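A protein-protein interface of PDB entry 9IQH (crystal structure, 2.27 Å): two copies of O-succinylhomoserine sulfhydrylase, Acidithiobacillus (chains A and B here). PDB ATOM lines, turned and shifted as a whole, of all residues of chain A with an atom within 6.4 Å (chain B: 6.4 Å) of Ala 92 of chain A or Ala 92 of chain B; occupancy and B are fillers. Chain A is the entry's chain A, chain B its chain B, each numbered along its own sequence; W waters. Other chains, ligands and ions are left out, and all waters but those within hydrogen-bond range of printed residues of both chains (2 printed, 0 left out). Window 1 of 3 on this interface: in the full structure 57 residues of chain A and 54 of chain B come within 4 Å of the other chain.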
ATOM      1  N   ALA A  90       1.623   4.055 -20.016  1.00  0.00           N
ATOM      2  CA  ALA A  90       0.578   4.859 -19.408  1.00  0.00           C
ATOM      3  C   ALA A  90       0.741   6.325 -19.790  1.00  0.00           C
ATOM      4  O   ALA A  90       1.830   6.783 -20.141  1.00  0.00           O
ATOM      5  CB  ALA A  90       0.603   4.703 -17.889  1.00  0.00           C
ATOM      6  N   THR A  91      -0.366   7.065 -19.714  1.00  0.00           N
ATOM      7  CA  THR A  91      -0.386   8.470 -20.100  1.00  0.00           C
ATOM      8  C   THR A  91      -1.221   9.270 -19.109  1.00  0.00           C
ATOM      9  O   THR A  91      -2.033   8.724 -18.358  1.00  0.00           O
ATOM     10  CB  THR A  91      -0.952   8.681 -21.509  1.00  0.00           C
ATOM     11  OG1 THR A  91      -2.307   8.216 -21.552  1.00  0.00           O
ATOM     12  CG2 THR A  91      -0.105   7.948 -22.563  1.00  0.00           C
ATOM     13  N   ALA A  92      -1.025  10.593 -19.149  1.00  0.00           N
ATOM     14  CA  ALA A  92      -1.666  11.484 -18.188  1.00  0.00           C
ATOM     15  C   ALA A  92      -3.185  11.451 -18.289  1.00  0.00           C
ATOM     16  O   ALA A  92      -3.872  11.726 -17.301  1.00  0.00           O
ATOM     17  CB  ALA A  92      -1.160  12.913 -18.387  1.00  0.00           C
ATOM     18  N   SER A  93      -3.729  11.133 -19.461  1.00  0.00           N
ATOM     19  CA  SER A  93      -5.175  11.068 -19.639  1.00  0.00           C
ATOM     20  C   SER A  93      -5.475  10.215 -20.861  1.00  0.00           C
ATOM     21  O   SER A  93      -4.576   9.839 -21.618  1.00  0.00           O
ATOM     22  CB  SER A  93      -5.796  12.460 -19.801  1.00  0.00           C
ATOM     23  OG  SER A  93      -5.465  13.010 -21.065  1.00  0.00           O
ATOM     24  N   GLY A  94      -6.765   9.916 -21.043  1.00  0.00           N
ATOM     25  CA  GLY A  94      -7.180   9.196 -22.234  1.00  0.00           C
ATOM     26  C   GLY A  94      -6.828   9.939 -23.509  1.00  0.00           C
ATOM     27  O   GLY A  94      -6.338   9.341 -24.471  1.00  0.00           O
ATOM     28  N   ALA A  96      -4.384  11.998 -23.921  1.00  0.00           N
ATOM     29  CA  ALA A  96      -2.942  11.882 -24.109  1.00  0.00           C
ATOM     30  C   ALA A  96      -2.557  10.518 -24.666  1.00  0.00           C
ATOM     31  O   ALA A  96      -1.560  10.407 -25.388  1.00  0.00           O
ATOM     32  CB  ALA A  96      -2.212  12.152 -22.791  1.00  0.00           C
ATOM     33  N   ALA A  97      -3.316   9.471 -24.331  1.00  0.00           N
ATOM     34  CA  ALA A  97      -3.091   8.167 -24.951  1.00  0.00           C
ATOM     35  C   ALA A  97      -3.407   8.207 -26.442  1.00  0.00           C
ATOM     36  O   ALA A  97      -2.682   7.615 -27.249  1.00  0.00           O
ATOM     37  CB  ALA A  97      -3.929   7.095 -24.253  1.00  0.00           C
ATOM     38  N   THR A 215      -9.537   6.956 -16.849  1.00  0.00           N
ATOM     39  CA  THR A 215     -10.488   7.854 -16.216  1.00  0.00           C
ATOM     40  C   THR A 215     -11.857   7.214 -16.042  1.00  0.00           C
ATOM     41  O   THR A 215     -12.562   7.497 -15.063  1.00  0.00           O
ATOM     42  CB  THR A 215     -10.618   9.112 -17.070  1.00  0.00           C
ATOM     43  OG1 THR A 215      -9.312   9.612 -17.388  1.00  0.00           O
ATOM     44  CG2 THR A 215     -11.418  10.166 -16.355  1.00  0.00           C
ATOM     45  N   LEU A 225      -7.757  11.172 -13.660  1.00  0.00           N
ATOM     46  CA  LEU A 225      -7.525  11.120 -15.095  1.00  0.00           C
ATOM     47  C   LEU A 225      -6.371  10.175 -15.376  1.00  0.00           C
ATOM     48  O   LEU A 225      -5.390  10.138 -14.628  1.00  0.00           O
ATOM     49  CB  LEU A 225      -7.204  12.502 -15.667  1.00  0.00           C
ATOM     50  CG  LEU A 225      -8.359  13.359 -16.184  1.00  0.00           C
ATOM     51  CD1 LEU A 225      -9.435  13.505 -15.134  1.00  0.00           C
ATOM     52  CD2 LEU A 225      -7.829  14.726 -16.591  1.00  0.00           C
ATOM     53  N   GLY A 226      -6.499   9.408 -16.449  1.00  0.00           N
ATOM     54  CA  GLY A 226      -5.421   8.544 -16.887  1.00  0.00           C
ATOM     55  C   GLY A 226      -5.755   7.919 -18.221  1.00  0.00           C
ATOM     56  O   GLY A 226      -6.921   7.871 -18.633  1.00  0.00           O
ATOM     57  N   GLY A 227      -4.707   7.438 -18.894  1.00  0.00           N
ATOM     58  CA  GLY A 227      -4.860   6.744 -20.156  1.00  0.00           C
ATOM     59  C   GLY A 227      -3.744   5.742 -20.340  1.00  0.00           C
ATOM     60  O   GLY A 227      -2.803   5.677 -19.546  1.00  0.00           O
ATOM     61  N   GLY A 248       6.533  13.889 -22.573  1.00  0.00           N
ATOM     62  CA  GLY A 248       6.114  13.920 -21.188  1.00  0.00           C
ATOM     63  C   GLY A 248       4.634  14.046 -20.837  1.00  0.00           C
ATOM     64  O   GLY A 248       4.293  14.701 -19.846  1.00  0.00           O
ATOM     65  N   PRO A 249       3.713  13.397 -21.586  1.00  0.00           N
ATOM     66  CA  PRO A 249       2.332  13.306 -21.070  1.00  0.00           C
ATOM     67  C   PRO A 249       2.184  12.165 -20.070  1.00  0.00           C
ATOM     68  O   PRO A 249       1.377  11.249 -20.243  1.00  0.00           O
ATOM     69  CB  PRO A 249       1.525  13.062 -22.350  1.00  0.00           C
ATOM     70  CG  PRO A 249       2.428  12.184 -23.145  1.00  0.00           C
ATOM     71  CD  PRO A 249       3.831  12.710 -22.886  1.00  0.00           C
ATOM     72  N   SER A 250       2.992  12.200 -19.016  1.00  0.00           N
ATOM     73  CA  SER A 250       3.132  11.032 -18.164  1.00  0.00           C
ATOM     74  C   SER A 250       2.066  11.003 -17.067  1.00  0.00           C
ATOM     75  O   SER A 250       1.425  12.006 -16.749  1.00  0.00           O
ATOM     76  CB  SER A 250       4.534  10.974 -17.554  1.00  0.00           C
ATOM     77  OG  SER A 250       4.868  12.189 -16.925  1.00  0.00           O
ATOM     78  N   LEU A 251       1.886   9.818 -16.493  1.00  0.00           N
ATOM     79  CA  LEU A 251       0.858   9.561 -15.497  1.00  0.00           C
ATOM     80  C   LEU A 251       1.458   9.679 -14.102  1.00  0.00           C
ATOM     81  O   LEU A 251       2.543   9.148 -13.836  1.00  0.00           O
ATOM     82  CB  LEU A 251       0.251   8.172 -15.707  1.00  0.00           C
ATOM     83  CG  LEU A 251      -0.837   7.694 -14.749  1.00  0.00           C
ATOM     84  CD1 LEU A 251      -2.051   8.596 -14.839  1.00  0.00           C
ATOM     85  CD2 LEU A 251      -1.211   6.241 -15.048  1.00  0.00           C
ATOM     86  N   SER A 252       0.758  10.383 -13.222  1.00  0.00           N
ATOM     87  CA  SER A 252       1.223  10.538 -11.859  1.00  0.00           C
ATOM     88  C   SER A 252       1.193   9.197 -11.128  1.00  0.00           C
ATOM     89  O   SER A 252       0.322   8.359 -11.387  1.00  0.00           O
ATOM     90  CB  SER A 252       0.357  11.543 -11.118  1.00  0.00           C
ATOM     91  OG  SER A 252       0.593  11.470  -9.730  1.00  0.00           O
ATOM     92  N   ASN A 255      -2.139   8.737  -9.348  1.00  0.00           N
ATOM     93  CA  ASN A 255      -3.205   8.326 -10.254  1.00  0.00           C
ATOM     94  C   ASN A 255      -3.043   6.868 -10.653  1.00  0.00           C
ATOM     95  O   ASN A 255      -4.025   6.122 -10.724  1.00  0.00           O
ATOM     96  CB  ASN A 255      -3.221   9.210 -11.502  1.00  0.00           C
ATOM     97  CG  ASN A 255      -3.683  10.621 -11.213  1.00  0.00           C
ATOM     98  OD1 ASN A 255      -3.369  11.187 -10.172  1.00  0.00           O
ATOM     99  ND2 ASN A 255      -4.436  11.196 -12.142  1.00  0.00           N
ATOM    100  N   GLN A 259      -5.628   3.765 -10.080  1.00  0.00           N
ATOM    101  CA  GLN A 259      -6.141   3.020 -11.220  1.00  0.00           C
ATOM    102  C   GLN A 259      -5.750   1.546 -11.163  1.00  0.00           C
ATOM    103  O   GLN A 259      -6.571   0.676 -11.476  1.00  0.00           O
ATOM    104  CB  GLN A 259      -5.664   3.687 -12.510  1.00  0.00           C
ATOM    105  CG  GLN A 259      -6.276   5.082 -12.700  1.00  0.00           C
ATOM    106  CD  GLN A 259      -5.443   5.977 -13.606  1.00  0.00           C
ATOM    107  OE1 GLN A 259      -4.471   5.534 -14.213  1.00  0.00           O
ATOM    108  NE2 GLN A 259      -5.823   7.243 -13.694  1.00  0.00           N
ATOM    109  N   ALA B  90      -1.319  24.469 -16.551  1.00  0.00           N
ATOM    110  CA  ALA B  90      -0.463  23.441 -15.991  1.00  0.00           C
ATOM    111  C   ALA B  90      -0.441  22.218 -16.893  1.00  0.00           C
ATOM    112  O   ALA B  90      -1.397  21.941 -17.622  1.00  0.00           O
ATOM    113  CB  ALA B  90      -0.936  23.047 -14.590  1.00  0.00           C
ATOM    114  N   THR B  91       0.664  21.476 -16.820  1.00  0.00           N
ATOM    115  CA  THR B  91       0.898  20.307 -17.651  1.00  0.00           C
ATOM    116  C   THR B  91       1.427  19.162 -16.797  1.00  0.00           C
ATOM    117  O   THR B  91       1.873  19.354 -15.663  1.00  0.00           O
ATOM    118  CB  THR B  91       1.900  20.603 -18.769  1.00  0.00           C
ATOM    119  OG1 THR B  91       3.139  21.024 -18.182  1.00  0.00           O
ATOM    120  CG2 THR B  91       1.379  21.696 -19.691  1.00  0.00           C
ATOM    121  N   ALA B  92       1.390  17.961 -17.374  1.00  0.00           N
ATOM    122  CA  ALA B  92       1.788  16.761 -16.647  1.00  0.00           C
ATOM    123  C   ALA B  92       3.259  16.764 -16.270  1.00  0.00           C
ATOM    124  O   ALA B  92       3.640  16.073 -15.319  1.00  0.00           O
ATOM    125  CB  ALA B  92       1.476  15.517 -17.478  1.00  0.00           C
ATOM    126  N   SER B  93       4.090  17.508 -16.996  1.00  0.00           N
ATOM    127  CA  SER B  93       5.524  17.554 -16.751  1.00  0.00           C
ATOM    128  C   SER B  93       6.080  18.792 -17.438  1.00  0.00           C
ATOM    129  O   SER B  93       5.396  19.449 -18.229  1.00  0.00           O
ATOM    130  CB  SER B  93       6.225  16.289 -17.259  1.00  0.00           C
ATOM    131  OG  SER B  93       6.065  16.174 -18.661  1.00  0.00           O
ATOM    132  N   GLY B  94       7.336  19.109 -17.116  1.00  0.00           N
ATOM    133  CA  GLY B  94       8.005  20.205 -17.796  1.00  0.00           C
ATOM    134  C   GLY B  94       8.125  19.963 -19.290  1.00  0.00           C
ATOM    135  O   GLY B  94       7.922  20.875 -20.096  1.00  0.00           O
ATOM    136  N   ALA B  96       6.035  18.201 -21.029  1.00  0.00           N
ATOM    137  CA  ALA B  96       4.708  18.452 -21.571  1.00  0.00           C
ATOM    138  C   ALA B  96       4.426  19.946 -21.673  1.00  0.00           C
ATOM    139  O   ALA B  96       3.637  20.368 -22.524  1.00  0.00           O
ATOM    140  CB  ALA B  96       3.643  17.750 -20.726  1.00  0.00           C
ATOM    141  N   ALA B  97       5.054  20.761 -20.819  1.00  0.00           N
ATOM    142  CA  ALA B  97       4.941  22.207 -20.978  1.00  0.00           C
ATOM    143  C   ALA B  97       5.667  22.677 -22.235  1.00  0.00           C
ATOM    144  O   ALA B  97       5.179  23.564 -22.944  1.00  0.00           O
ATOM    145  CB  ALA B  97       5.479  22.924 -19.738  1.00  0.00           C
ATOM    146  N   THR B 215       8.546  19.962 -11.502  1.00  0.00           N
ATOM    147  CA  THR B 215       9.344  18.873 -10.963  1.00  0.00           C
ATOM    148  C   THR B 215      10.562  19.374 -10.198  1.00  0.00           C
ATOM    149  O   THR B 215      11.010  18.709  -9.254  1.00  0.00           O
ATOM    150  CB  THR B 215       9.785  17.968 -12.114  1.00  0.00           C
ATOM    151  OG1 THR B 215       8.652  17.641 -12.926  1.00  0.00           O
ATOM    152  CG2 THR B 215      10.430  16.707 -11.596  1.00  0.00           C
ATOM    153  N   LEU B 225       6.092  15.045 -10.713  1.00  0.00           N
ATOM    154  CA  LEU B 225       6.290  15.628 -12.031  1.00  0.00           C
ATOM    155  C   LEU B 225       5.200  16.656 -12.302  1.00  0.00           C
ATOM    156  O   LEU B 225       4.036  16.456 -11.939  1.00  0.00           O
ATOM    157  CB  LEU B 225       6.256  14.556 -13.126  1.00  0.00           C
ATOM    158  CG  LEU B 225       7.546  13.866 -13.574  1.00  0.00           C
ATOM    159  CD1 LEU B 225       8.422  13.494 -12.404  1.00  0.00           C
ATOM    160  CD2 LEU B 225       7.208  12.621 -14.396  1.00  0.00           C
ATOM    161  N   GLY B 226       5.582  17.756 -12.938  1.00  0.00           N
ATOM    162  CA  GLY B 226       4.610  18.748 -13.353  1.00  0.00           C
ATOM    163  C   GLY B 226       5.280  19.830 -14.162  1.00  0.00           C
ATOM    164  O   GLY B 226       6.494  20.042 -14.069  1.00  0.00           O
ATOM    165  N   GLY B 227       4.466  20.526 -14.957  1.00  0.00           N
ATOM    166  CA  GLY B 227       4.945  21.652 -15.730  1.00  0.00           C
ATOM    167  C   GLY B 227       3.897  22.747 -15.812  1.00  0.00           C
ATOM    168  O   GLY B 227       2.772  22.597 -15.325  1.00  0.00           O
ATOM    169  N   GLY B 248      -4.604  16.618 -23.891  1.00  0.00           N
ATOM    170  CA  GLY B 248      -4.664  16.064 -22.554  1.00  0.00           C
ATOM    171  C   GLY B 248      -3.390  15.752 -21.777  1.00  0.00           C
ATOM    172  O   GLY B 248      -3.373  14.793 -20.998  1.00  0.00           O
ATOM    173  N   PRO B 249      -2.302  16.549 -21.914  1.00  0.00           N
ATOM    174  CA  PRO B 249      -1.191  16.354 -20.964  1.00  0.00           C
ATOM    175  C   PRO B 249      -1.438  17.095 -19.655  1.00  0.00           C
ATOM    176  O   PRO B 249      -0.666  17.963 -19.242  1.00  0.00           O
ATOM    177  CB  PRO B 249       0.006  16.915 -21.741  1.00  0.00           C
ATOM    178  CG  PRO B 249      -0.584  18.048 -22.486  1.00  0.00           C
ATOM    179  CD  PRO B 249      -1.976  17.608 -22.889  1.00  0.00           C
ATOM    180  N   SER B 250      -2.541  16.763 -18.997  1.00  0.00           N
ATOM    181  CA  SER B 250      -2.980  17.561 -17.868  1.00  0.00           C
ATOM    182  C   SER B 250      -2.287  17.124 -16.579  1.00  0.00           C
ATOM    183  O   SER B 250      -1.718  16.035 -16.473  1.00  0.00           O
ATOM    184  CB  SER B 250      -4.498  17.486 -17.721  1.00  0.00           C
ATOM    185  OG  SER B 250      -4.949  16.157 -17.833  1.00  0.00           O
ATOM    186  N   LEU B 251      -2.334  18.011 -15.594  1.00  0.00           N
ATOM    187  CA  LEU B 251      -1.649  17.822 -14.327  1.00  0.00           C
ATOM    188  C   LEU B 251      -2.613  17.206 -13.325  1.00  0.00           C
ATOM    189  O   LEU B 251      -3.756  17.656 -13.200  1.00  0.00           O
ATOM    190  CB  LEU B 251      -1.112  19.152 -13.797  1.00  0.00           C
ATOM    191  CG  LEU B 251      -0.355  19.094 -12.472  1.00  0.00           C
ATOM    192  CD1 LEU B 251       0.895  18.256 -12.633  1.00  0.00           C
ATOM    193  CD2 LEU B 251      -0.020  20.493 -11.976  1.00  0.00           C
ATOM    194  N   SER B 252      -2.153  16.175 -12.634  1.00  0.00           N
ATOM    195  CA  SER B 252      -2.964  15.546 -11.609  1.00  0.00           C
ATOM    196  C   SER B 252      -3.181  16.508 -10.443  1.00  0.00           C
ATOM    197  O   SER B 252      -2.254  17.222 -10.046  1.00  0.00           O
ATOM    198  CB  SER B 252      -2.290  14.276 -11.102  1.00  0.00           C
ATOM    199  OG  SER B 252      -3.001  13.756  -9.995  1.00  0.00           O
ATOM    200  N   ASN B 255      -0.610  16.026  -7.716  1.00  0.00           N
ATOM    201  CA  ASN B 255       0.642  16.711  -8.021  1.00  0.00           C
ATOM    202  C   ASN B 255       0.494  18.220  -7.879  1.00  0.00           C
ATOM    203  O   ASN B 255       1.370  18.887  -7.311  1.00  0.00           O
ATOM    204  CB  ASN B 255       1.103  16.346  -9.433  1.00  0.00           C
ATOM    205  CG  ASN B 255       1.486  14.877  -9.561  1.00  0.00           C
ATOM    206  OD1 ASN B 255       0.958  14.024  -8.852  1.00  0.00           O
ATOM    207  ND2 ASN B 255       2.416  14.581 -10.467  1.00  0.00           N
ATOM    208  N   GLN B 259       2.609  20.755  -5.484  1.00  0.00           N
ATOM    209  CA  GLN B 259       3.383  21.832  -6.085  1.00  0.00           C
ATOM    210  C   GLN B 259       2.915  23.206  -5.612  1.00  0.00           C
ATOM    211  O   GLN B 259       3.740  24.088  -5.355  1.00  0.00           O
ATOM    212  CB  GLN B 259       3.329  21.701  -7.612  1.00  0.00           C
ATOM    213  CG  GLN B 259       4.063  20.434  -8.092  1.00  0.00           C
ATOM    214  CD  GLN B 259       3.554  19.879  -9.413  1.00  0.00           C
ATOM    215  OE1 GLN B 259       2.792  20.529 -10.131  1.00  0.00           O
ATOM    216  NE2 GLN B 259       3.982  18.665  -9.739  1.00  0.00           N
HETATM  217  O   HOH W   1       2.622  13.790 -14.247  1.00  0.00           O
HETATM  218  O   HOH W   2      -3.437  13.424 -15.356  1.00  0.00           O
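OG of Ser 252 of chain A is in hydrogen-bond range of OD1 of Asn 255 of chain B.
The side-chain hydroxyl of Ser 93 of chain A lies within hydrogen-bond range of the backbone carbonyl oxygen of Gly 248 of chain B, 2.7 Å away.
OG of Ser 93 of chain B sits at hydrogen-bond distance from O of Gly 248 of chain A, 2.6 Å away.
OD1 of Asn 255 of chain A is in hydrogen-bond range of OG of Ser 252 of chain B (2.6 Å).
N of Ala 92 of chain B sits at hydrogen-bond distance from O of Pro 249 of chain B, at 2.8 Å.
The side-chain hydroxyl (OG) of Ser 93 of chain B lies within hydrogen-bond range of the backbone NH (N) of Ala 96 of chain B, at 3.1 Å.
The side-chain hydroxyl of Ser 93 of chain A sits at hydrogen-bond distance from the backbone NH of Ala 96 of chain A, at 3.2 Å.
NE2 of Gln 259 of chain B is in hydrogen-bond range of O of Leu 225 of chain B, at 3.1 Å.
The backbone NH of Ala 92 of chain A lies within hydrogen-bond range of the backbone carbonyl oxygen of Pro 249 of chain A (2.7 Å).
The backbone carbonyl oxygen (O) of Leu 225 of chain A is in hydrogen-bond range of the side-chain amide nitrogen (ND2) of Asn 255 of chain A (2.9 Å).
Among the printed residues, pairs that only touch across the chains: Gly 248 of chain A with Ala 96 of chain B (3.2 Å), Ala 96 of chain A with Gly 248 of chain B (3.4 Å), Leu 225 of chain A with Ser 250 of chain B (3.4 Å), Ser 250 of chain A with Leu 225 of chain B (3.5 Å), Ser 250 of chain A with Ala 92 of chain B (3.6 Å), Ala 92 of chain A with Ser 250 of chain B (3.7 Å), Gly 248 of chain A with Ala 92 of chain B (3.8 Å), Ser 252 of chain A with Ser 252 of chain B (3.8 Å), Ala 92 of chain A with Ala 92 of chain B (3.8 Å) and Ala 92 of chain A with Gly 248 of chain B (3.9 Å).
Ala 92 of chain A touches three residues of chain B.
Of the printed residues of chain B, Ala 96 of chain A touches Gly 248 (3.4 Å).
Gly 226 of chain A touches none of the printed residues of chain B.
Of chain A, only Ala 92 (3.8 Å), Gly 248 (3.8 Å) and Ser 250 (3.6 Å) come within 4 Å of Ala 92 of chain B.
Of the printed residues of chain A, Asn 255 of chain B touches Ser 252 (2.7 Å).
The nearest residue of chain B that does not touch Ala 92 of chain A is Pro 249 of chain B (4.3 Å).
Hydrophobic or aromatic side chains of chain B within 4 Å of the printed part of chain A: Ala 92, Ala 96 and Leu 225.
Of the 18 printed residues of chain A, 8 touch a printed residue of chain B.
Among the printed residues, no Asp or Glu carboxylate lies within 4 Å of a Lys or Arg side-chain nitrogen of the other chain.
Ala 92 of chain A touches Gly 248 of chain B, and with the chains exchanged Gly 248 of chain A touches Ala 92 of chain B.
Ser 93 of chain A touches Gly 248 of chain B, and with the chains exchanged Gly 248 of chain A touches Ser 93 of chain B.
Ala 96 of chain A touches Gly 248 of chain B, and with the chains exchanged Gly 248 of chain A touches Ala 96 of chain B.
Ser 252 of chain A touches its own counterpart, Ser 252 of chain B.
Positions printed for both chains: 90, 91, 92, 93, 94, 96, 97, 215, 225, 226, 227, 248, 249, 250, 251, 252, 255 and 259.
Water W2 lies within hydrogen-bond range of the backbone carbonyl oxygen (O) of Ala 92 of chain A and the backbone carbonyl oxygen (O) of Ser 250 of chain B.
Water W1 lies within hydrogen-bond range of O of Ala 92 of chain B (2.7 Å) and O of Ser 250 of chain A (3.3 Å).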
